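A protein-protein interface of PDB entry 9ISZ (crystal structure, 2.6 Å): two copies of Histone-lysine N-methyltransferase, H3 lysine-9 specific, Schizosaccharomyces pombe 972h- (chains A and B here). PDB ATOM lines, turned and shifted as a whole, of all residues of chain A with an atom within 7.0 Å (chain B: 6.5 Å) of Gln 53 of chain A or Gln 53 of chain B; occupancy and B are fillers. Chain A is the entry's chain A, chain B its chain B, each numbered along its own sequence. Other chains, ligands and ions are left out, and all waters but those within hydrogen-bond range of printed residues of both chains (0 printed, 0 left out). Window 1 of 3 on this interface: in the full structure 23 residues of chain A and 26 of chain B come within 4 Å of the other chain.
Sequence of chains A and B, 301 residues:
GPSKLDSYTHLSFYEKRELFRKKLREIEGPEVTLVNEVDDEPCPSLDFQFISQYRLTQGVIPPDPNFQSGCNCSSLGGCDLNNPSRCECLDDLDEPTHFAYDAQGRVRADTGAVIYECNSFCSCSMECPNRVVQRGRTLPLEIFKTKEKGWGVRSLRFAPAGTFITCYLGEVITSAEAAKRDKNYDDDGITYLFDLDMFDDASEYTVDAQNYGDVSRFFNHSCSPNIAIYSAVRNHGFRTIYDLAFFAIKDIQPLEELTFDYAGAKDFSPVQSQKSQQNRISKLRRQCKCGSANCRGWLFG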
ATOM      1  N   GLU A  28     -21.995  23.662  -0.920  1.00  0.00           N
ATOM      2  CA  GLU A  28     -23.190  24.010  -1.676  1.00  0.00           C
ATOM      3  C   GLU A  28     -22.924  25.191  -2.602  1.00  0.00           C
ATOM      4  O   GLU A  28     -22.240  26.151  -2.233  1.00  0.00           O
ATOM      5  CB  GLU A  28     -24.331  24.340  -0.713  1.00  0.00           C
ATOM      6  CG  GLU A  28     -25.665  24.617  -1.379  1.00  0.00           C
ATOM      7  CD  GLU A  28     -26.775  24.840  -0.372  1.00  0.00           C
ATOM      8  OE1 GLU A  28     -26.611  25.707   0.513  1.00  0.00           O
ATOM      9  OE2 GLU A  28     -27.803  24.139  -0.458  1.00  0.00           O
ATOM     10  N   PHE A  50     -16.670  22.316   6.673  1.00  0.00           N
ATOM     11  CA  PHE A  50     -17.470  23.372   6.067  1.00  0.00           C
ATOM     12  C   PHE A  50     -18.932  23.254   6.478  1.00  0.00           C
ATOM     13  O   PHE A  50     -19.472  22.151   6.607  1.00  0.00           O
ATOM     14  CB  PHE A  50     -17.352  23.333   4.543  1.00  0.00           C
ATOM     15  CG  PHE A  50     -16.098  23.969   4.018  1.00  0.00           C
ATOM     16  CD1 PHE A  50     -16.004  25.347   3.902  1.00  0.00           C
ATOM     17  CD2 PHE A  50     -15.013  23.194   3.643  1.00  0.00           C
ATOM     18  CE1 PHE A  50     -14.852  25.941   3.421  1.00  0.00           C
ATOM     19  CE2 PHE A  50     -13.857  23.783   3.160  1.00  0.00           C
ATOM     20  CZ  PHE A  50     -13.779  25.159   3.049  1.00  0.00           C
ATOM     21  N   ILE A  51     -19.569  24.406   6.685  1.00  0.00           N
ATOM     22  CA  ILE A  51     -20.966  24.473   7.084  1.00  0.00           C
ATOM     23  C   ILE A  51     -21.684  25.473   6.189  1.00  0.00           C
ATOM     24  O   ILE A  51     -21.076  26.374   5.609  1.00  0.00           O
ATOM     25  CB  ILE A  51     -21.123  24.861   8.568  1.00  0.00           C
ATOM     26  CG1 ILE A  51     -20.497  26.233   8.823  1.00  0.00           C
ATOM     27  CG2 ILE A  51     -20.488  23.806   9.465  1.00  0.00           C
ATOM     28  CD1 ILE A  51     -20.598  26.686  10.261  1.00  0.00           C
ATOM     29  N   SER A  52     -23.000  25.303   6.081  1.00  0.00           N
ATOM     30  CA  SER A  52     -23.819  26.147   5.221  1.00  0.00           C
ATOM     31  C   SER A  52     -24.640  27.173   5.990  1.00  0.00           C
ATOM     32  O   SER A  52     -25.391  27.930   5.367  1.00  0.00           O
ATOM     33  CB  SER A  52     -24.752  25.285   4.364  1.00  0.00           C
ATOM     34  OG  SER A  52     -25.647  24.545   5.173  1.00  0.00           O
ATOM     35  N   GLN A  53     -24.515  27.226   7.313  1.00  0.00           N
ATOM     36  CA  GLN A  53     -25.298  28.157   8.116  1.00  0.00           C
ATOM     37  C   GLN A  53     -24.686  28.240   9.508  1.00  0.00           C
ATOM     38  O   GLN A  53     -23.755  27.502   9.847  1.00  0.00           O
ATOM     39  CB  GLN A  53     -26.766  27.734   8.186  1.00  0.00           C
ATOM     40  CG  GLN A  53     -26.964  26.275   8.558  1.00  0.00           C
ATOM     41  CD  GLN A  53     -28.395  25.819   8.367  1.00  0.00           C
ATOM     42  OE1 GLN A  53     -28.674  24.620   8.305  1.00  0.00           O
ATOM     43  NE2 GLN A  53     -29.314  26.774   8.271  1.00  0.00           N
ATOM     44  N   TYR A  54     -25.227  29.154  10.313  1.00  0.00           N
ATOM     45  CA  TYR A  54     -24.752  29.332  11.679  1.00  0.00           C
ATOM     46  C   TYR A  54     -24.920  28.053  12.484  1.00  0.00           C
ATOM     47  O   TYR A  54     -25.937  27.359  12.381  1.00  0.00           O
ATOM     48  CB  TYR A  54     -25.509  30.468  12.368  1.00  0.00           C
ATOM     49  CG  TYR A  54     -24.990  31.851  12.056  1.00  0.00           C
ATOM     50  CD1 TYR A  54     -23.774  32.032  11.410  1.00  0.00           C
ATOM     51  CD2 TYR A  54     -25.714  32.978  12.416  1.00  0.00           C
ATOM     52  CE1 TYR A  54     -23.298  33.299  11.125  1.00  0.00           C
ATOM     53  CE2 TYR A  54     -25.248  34.246  12.139  1.00  0.00           C
ATOM     54  CZ  TYR A  54     -24.040  34.403  11.492  1.00  0.00           C
ATOM     55  OH  TYR A  54     -23.573  35.668  11.215  1.00  0.00           O
ATOM     56  N   ARG A  55     -23.913  27.748  13.292  1.00  0.00           N
ATOM     57  CA  ARG A  55     -23.951  26.641  14.241  1.00  0.00           C
ATOM     58  C   ARG A  55     -23.972  27.264  15.633  1.00  0.00           C
ATOM     59  O   ARG A  55     -22.929  27.611  16.190  1.00  0.00           O
ATOM     60  CB  ARG A  55     -22.757  25.714  14.058  1.00  0.00           C
ATOM     61  CG  ARG A  55     -23.050  24.264  14.394  1.00  0.00           C
ATOM     62  CD  ARG A  55     -21.799  23.527  14.845  1.00  0.00           C
ATOM     63  NE  ARG A  55     -21.595  23.642  16.284  1.00  0.00           N
ATOM     64  CZ  ARG A  55     -22.208  22.889  17.187  1.00  0.00           C
ATOM     65  NH1 ARG A  55     -23.078  21.957  16.833  1.00  0.00           N
ATOM     66  NH2 ARG A  55     -21.945  23.077  18.477  1.00  0.00           N
ATOM     67  N   LEU A  56     -25.172  27.422  16.184  1.00  0.00           N
ATOM     68  CA  LEU A  56     -25.314  27.995  17.513  1.00  0.00           C
ATOM     69  C   LEU A  56     -24.779  27.034  18.569  1.00  0.00           C
ATOM     70  O   LEU A  56     -24.774  25.814  18.385  1.00  0.00           O
ATOM     71  CB  LEU A  56     -26.780  28.324  17.794  1.00  0.00           C
ATOM     72  CG  LEU A  56     -27.521  29.021  16.653  1.00  0.00           C
ATOM     73  CD1 LEU A  56     -28.999  29.140  16.971  1.00  0.00           C
ATOM     74  CD2 LEU A  56     -26.918  30.386  16.375  1.00  0.00           C
ATOM     75  N   LEU A 169     -19.718  32.478   8.197  1.00  0.00           N
ATOM     76  CA  LEU A 169     -20.365  31.463   9.010  1.00  0.00           C
ATOM     77  C   LEU A 169     -19.372  30.874  10.000  1.00  0.00           C
ATOM     78  O   LEU A 169     -18.163  31.104   9.920  1.00  0.00           O
ATOM     79  CB  LEU A 169     -20.959  30.360   8.125  1.00  0.00           C
ATOM     80  CG  LEU A 169     -21.944  30.829   7.051  1.00  0.00           C
ATOM     81  CD1 LEU A 169     -22.366  29.667   6.173  1.00  0.00           C
ATOM     82  CD2 LEU A 169     -23.157  31.496   7.683  1.00  0.00           C
ATOM     83  N   GLY A 170     -19.905  30.109  10.944  1.00  0.00           N
ATOM     84  CA  GLY A 170     -19.083  29.490  11.968  1.00  0.00           C
ATOM     85  C   GLY A 170     -19.923  29.157  13.188  1.00  0.00           C
ATOM     86  O   GLY A 170     -21.148  29.091  13.116  1.00  0.00           O
ATOM     87  N   GLU A 171     -19.229  28.948  14.304  1.00  0.00           N
ATOM     88  CA  GLU A 171     -19.882  28.703  15.585  1.00  0.00           C
ATOM     89  C   GLU A 171     -20.293  30.031  16.208  1.00  0.00           C
ATOM     90  O   GLU A 171     -19.443  30.891  16.453  1.00  0.00           O
ATOM     91  CB  GLU A 171     -18.945  27.953  16.531  1.00  0.00           C
ATOM     92  CG  GLU A 171     -18.638  26.518  16.152  1.00  0.00           C
ATOM     93  CD  GLU A 171     -17.723  25.842  17.160  1.00  0.00           C
ATOM     94  OE1 GLU A 171     -16.573  26.306  17.328  1.00  0.00           O
ATOM     95  OE2 GLU A 171     -18.157  24.858  17.797  1.00  0.00           O
ATOM     96  N   VAL A 172     -21.582  30.202  16.474  1.00  0.00           N
ATOM     97  CA  VAL A 172     -22.033  31.362  17.237  1.00  0.00           C
ATOM     98  C   VAL A 172     -21.836  31.052  18.714  1.00  0.00           C
ATOM     99  O   VAL A 172     -22.385  30.074  19.231  1.00  0.00           O
ATOM    100  CB  VAL A 172     -23.496  31.706  16.928  1.00  0.00           C
ATOM    101  CG1 VAL A 172     -23.872  33.025  17.584  1.00  0.00           C
ATOM    102  CG2 VAL A 172     -23.713  31.778  15.427  1.00  0.00           C
ATOM    103  N   TYR A 212     -15.292  25.560  12.311  1.00  0.00           N
ATOM    104  CA  TYR A 212     -16.383  25.471  11.353  1.00  0.00           C
ATOM    105  C   TYR A 212     -16.625  26.855  10.773  1.00  0.00           C
ATOM    106  O   TYR A 212     -16.431  27.865  11.453  1.00  0.00           O
ATOM    107  CB  TYR A 212     -17.671  24.940  11.998  1.00  0.00           C
ATOM    108  CG  TYR A 212     -17.477  23.691  12.828  1.00  0.00           C
ATOM    109  CD1 TYR A 212     -17.161  23.773  14.179  1.00  0.00           C
ATOM    110  CD2 TYR A 212     -17.611  22.431  12.263  1.00  0.00           C
ATOM    111  CE1 TYR A 212     -16.982  22.636  14.942  1.00  0.00           C
ATOM    112  CE2 TYR A 212     -17.433  21.285  13.019  1.00  0.00           C
ATOM    113  CZ  TYR A 212     -17.120  21.395  14.357  1.00  0.00           C
ATOM    114  OH  TYR A 212     -16.943  20.257  15.111  1.00  0.00           O
ATOM    115  N   GLY A 213     -17.055  26.899   9.518  1.00  0.00           N
ATOM    116  CA  GLY A 213     -17.288  28.179   8.873  1.00  0.00           C
ATOM    117  C   GLY A 213     -17.436  28.020   7.368  1.00  0.00           C
ATOM    118  O   GLY A 213     -17.696  26.929   6.863  1.00  0.00           O
ATOM    119  N   ASP A 214     -17.260  29.141   6.678  1.00  0.00           N
ATOM    120  CA  ASP A 214     -17.484  29.276   5.246  1.00  0.00           C
ATOM    121  C   ASP A 214     -16.172  29.645   4.556  1.00  0.00           C
ATOM    122  O   ASP A 214     -15.129  29.779   5.193  1.00  0.00           O
ATOM    123  CB  ASP A 214     -18.570  30.324   4.980  1.00  0.00           C
ATOM    124  CG  ASP A 214     -19.115  30.255   3.575  1.00  0.00           C
ATOM    125  OD1 ASP A 214     -19.712  29.216   3.223  1.00  0.00           O
ATOM    126  OD2 ASP A 214     -18.939  31.238   2.822  1.00  0.00           O
ATOM    127  N   ARG A 234     -33.506  38.726   9.014  1.00  0.00           N
ATOM    128  CA  ARG A 234     -34.759  38.090   8.637  1.00  0.00           C
ATOM    129  C   ARG A 234     -35.813  38.159   9.729  1.00  0.00           C
ATOM    130  O   ARG A 234     -37.002  38.261   9.418  1.00  0.00           O
ATOM    131  CB  ARG A 234     -34.523  36.625   8.243  1.00  0.00           C
ATOM    132  CG  ARG A 234     -33.988  36.466   6.824  1.00  0.00           C
ATOM    133  CD  ARG A 234     -33.757  35.010   6.443  1.00  0.00           C
ATOM    134  NE  ARG A 234     -32.564  34.455   7.068  1.00  0.00           N
ATOM    135  CZ  ARG A 234     -32.571  33.680   8.144  1.00  0.00           C
ATOM    136  NH1 ARG A 234     -33.700  33.336   8.739  1.00  0.00           N
ATOM    137  NH2 ARG A 234     -31.416  33.238   8.633  1.00  0.00           N
ATOM    138  N   ILE B  51     -32.500  22.528  -2.181  1.00  0.00           N
ATOM    139  CA  ILE B  51     -32.310  23.286  -0.952  1.00  0.00           C
ATOM    140  C   ILE B  51     -31.710  22.365   0.093  1.00  0.00           C
ATOM    141  O   ILE B  51     -32.007  21.167   0.135  1.00  0.00           O
ATOM    142  CB  ILE B  51     -33.629  23.904  -0.438  1.00  0.00           C
ATOM    143  CG1 ILE B  51     -34.708  22.824  -0.330  1.00  0.00           C
ATOM    144  CG2 ILE B  51     -34.072  25.034  -1.344  1.00  0.00           C
ATOM    145  CD1 ILE B  51     -36.027  23.339   0.186  1.00  0.00           C
ATOM    146  N   SER B  52     -30.858  22.929   0.940  1.00  0.00           N
ATOM    147  CA  SER B  52     -30.178  22.150   1.964  1.00  0.00           C
ATOM    148  C   SER B  52     -30.934  22.120   3.285  1.00  0.00           C
ATOM    149  O   SER B  52     -30.434  21.534   4.253  1.00  0.00           O
ATOM    150  CB  SER B  52     -28.759  22.692   2.183  1.00  0.00           C
ATOM    151  OG  SER B  52     -28.783  24.072   2.505  1.00  0.00           O
ATOM    152  N   GLN B  53     -32.118  22.728   3.350  1.00  0.00           N
ATOM    153  CA  GLN B  53     -32.926  22.723   4.564  1.00  0.00           C
ATOM    154  C   GLN B  53     -34.344  23.158   4.214  1.00  0.00           C
ATOM    155  O   GLN B  53     -34.627  23.585   3.092  1.00  0.00           O
ATOM    156  CB  GLN B  53     -32.330  23.633   5.641  1.00  0.00           C
ATOM    157  CG  GLN B  53     -32.273  25.096   5.248  1.00  0.00           C
ATOM    158  CD  GLN B  53     -31.722  25.967   6.353  1.00  0.00           C
ATOM    159  OE1 GLN B  53     -31.251  25.466   7.374  1.00  0.00           O
ATOM    160  NE2 GLN B  53     -31.780  27.279   6.161  1.00  0.00           N
ATOM    161  N   TYR B  54     -35.232  23.049   5.203  1.00  0.00           N
ATOM    162  CA  TYR B  54     -36.626  23.430   5.013  1.00  0.00           C
ATOM    163  C   TYR B  54     -36.748  24.910   4.674  1.00  0.00           C
ATOM    164  O   TYR B  54     -36.039  25.756   5.227  1.00  0.00           O
ATOM    165  CB  TYR B  54     -37.437  23.138   6.275  1.00  0.00           C
ATOM    166  CG  TYR B  54     -37.995  21.738   6.384  1.00  0.00           C
ATOM    167  CD1 TYR B  54     -38.261  20.981   5.252  1.00  0.00           C
ATOM    168  CD2 TYR B  54     -38.269  21.179   7.629  1.00  0.00           C
ATOM    169  CE1 TYR B  54     -38.779  19.700   5.356  1.00  0.00           C
ATOM    170  CE2 TYR B  54     -38.786  19.900   7.743  1.00  0.00           C
ATOM    171  CZ  TYR B  54     -39.038  19.166   6.604  1.00  0.00           C
ATOM    172  OH  TYR B  54     -39.553  17.894   6.717  1.00  0.00           O
ATOM    173  N   ARG B  55     -37.665  25.217   3.762  1.00  0.00           N
ATOM    174  CA  ARG B  55     -38.066  26.587   3.462  1.00  0.00           C
ATOM    175  C   ARG B  55     -39.500  26.767   3.946  1.00  0.00           C
ATOM    176  O   ARG B  55     -40.436  26.221   3.352  1.00  0.00           O
ATOM    177  CB  ARG B  55     -37.944  26.881   1.970  1.00  0.00           C
ATOM    178  CG  ARG B  55     -36.527  26.822   1.452  1.00  0.00           C
ATOM    179  CD  ARG B  55     -35.713  28.016   1.919  1.00  0.00           C
ATOM    180  NE  ARG B  55     -34.337  27.941   1.440  1.00  0.00           N
ATOM    181  CZ  ARG B  55     -33.963  28.206   0.196  1.00  0.00           C
ATOM    182  NH1 ARG B  55     -34.841  28.553  -0.732  1.00  0.00           N
ATOM    183  NH2 ARG B  55     -32.676  28.118  -0.128  1.00  0.00           N
ATOM    184  N   LEU B 169     -36.920  17.228   1.931  1.00  0.00           N
ATOM    185  CA  LEU B 169     -36.947  18.668   2.112  1.00  0.00           C
ATOM    186  C   LEU B 169     -37.866  19.307   1.079  1.00  0.00           C
ATOM    187  O   LEU B 169     -38.285  18.677   0.105  1.00  0.00           O
ATOM    188  CB  LEU B 169     -35.533  19.252   2.014  1.00  0.00           C
ATOM    189  CG  LEU B 169     -34.547  18.739   3.064  1.00  0.00           C
ATOM    190  CD1 LEU B 169     -33.165  19.334   2.846  1.00  0.00           C
ATOM    191  CD2 LEU B 169     -35.060  19.061   4.454  1.00  0.00           C
ATOM    192  N   GLY B 170     -38.173  20.573   1.315  1.00  0.00           N
ATOM    193  CA  GLY B 170     -39.055  21.318   0.442  1.00  0.00           C
ATOM    194  C   GLY B 170     -39.676  22.471   1.205  1.00  0.00           C
ATOM    195  O   GLY B 170     -39.242  22.819   2.304  1.00  0.00           O
ATOM    196  N   GLY B 213     -36.652  21.384  -3.073  1.00  0.00           N
ATOM    197  CA  GLY B 213     -36.557  20.134  -2.333  1.00  0.00           C
ATOM    198  C   GLY B 213     -35.168  19.535  -2.372  1.00  0.00           C
ATOM    199  O   GLY B 213     -34.161  20.253  -2.399  1.00  0.00           O
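The side-chain amide nitrogen (NE2) of Gln 53 of chain A sits at hydrogen-bond distance from the side-chain amide oxygen (OE1) of Gln 53 of chain B (2.5 Å).
The side-chain carboxylate (OE2) of Glu 28 of chain A lies within hydrogen-bond range of the side-chain hydroxyl (OG) of Ser 52 of chain B.
Of the printed residues of chain B, Glu 28 of chain A touches Ser 52.
Of chain B, only Gln 53 comes within 4 Å of Gln 53 of chain A.
Asp 214 of chain A touches none of the printed residues of chain B.
Of the printed residues of chain A, Ser 52 of chain B touches Glu 28.
Of chain A, only Gln 53 (2.5 Å) comes within 4 Å of Gln 53 of chain B.
Gly 170 of chain B touches none of the printed residues of chain A.
The nearest residue of chain A that does not touch Gln 53 of chain B is Glu 28 of chain A (5.9 Å).
The nearest printed residue of chain B that does not touch Glu 28 of chain A is Ile 51 of chain B (4.3 Å).
Of the 16 printed residues of chain A, 2 touch a printed residue of chain B.
Printed residues of chain A that touch a printed residue of chain B: Glu 28 and Gln 53.
Among the printed residues, 2 pairs touch across the chains.
Among the printed residues, no Asp or Glu carboxylate lies within 4 Å of a Lys or Arg side-chain nitrogen of the other chain.
Gln 53 of chain B touches its own counterpart, Gln 53 of chain A.
Of the 2 pairs that touch across the chains among the printed residues, 1 has its exchanged pair printed and touching as well.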
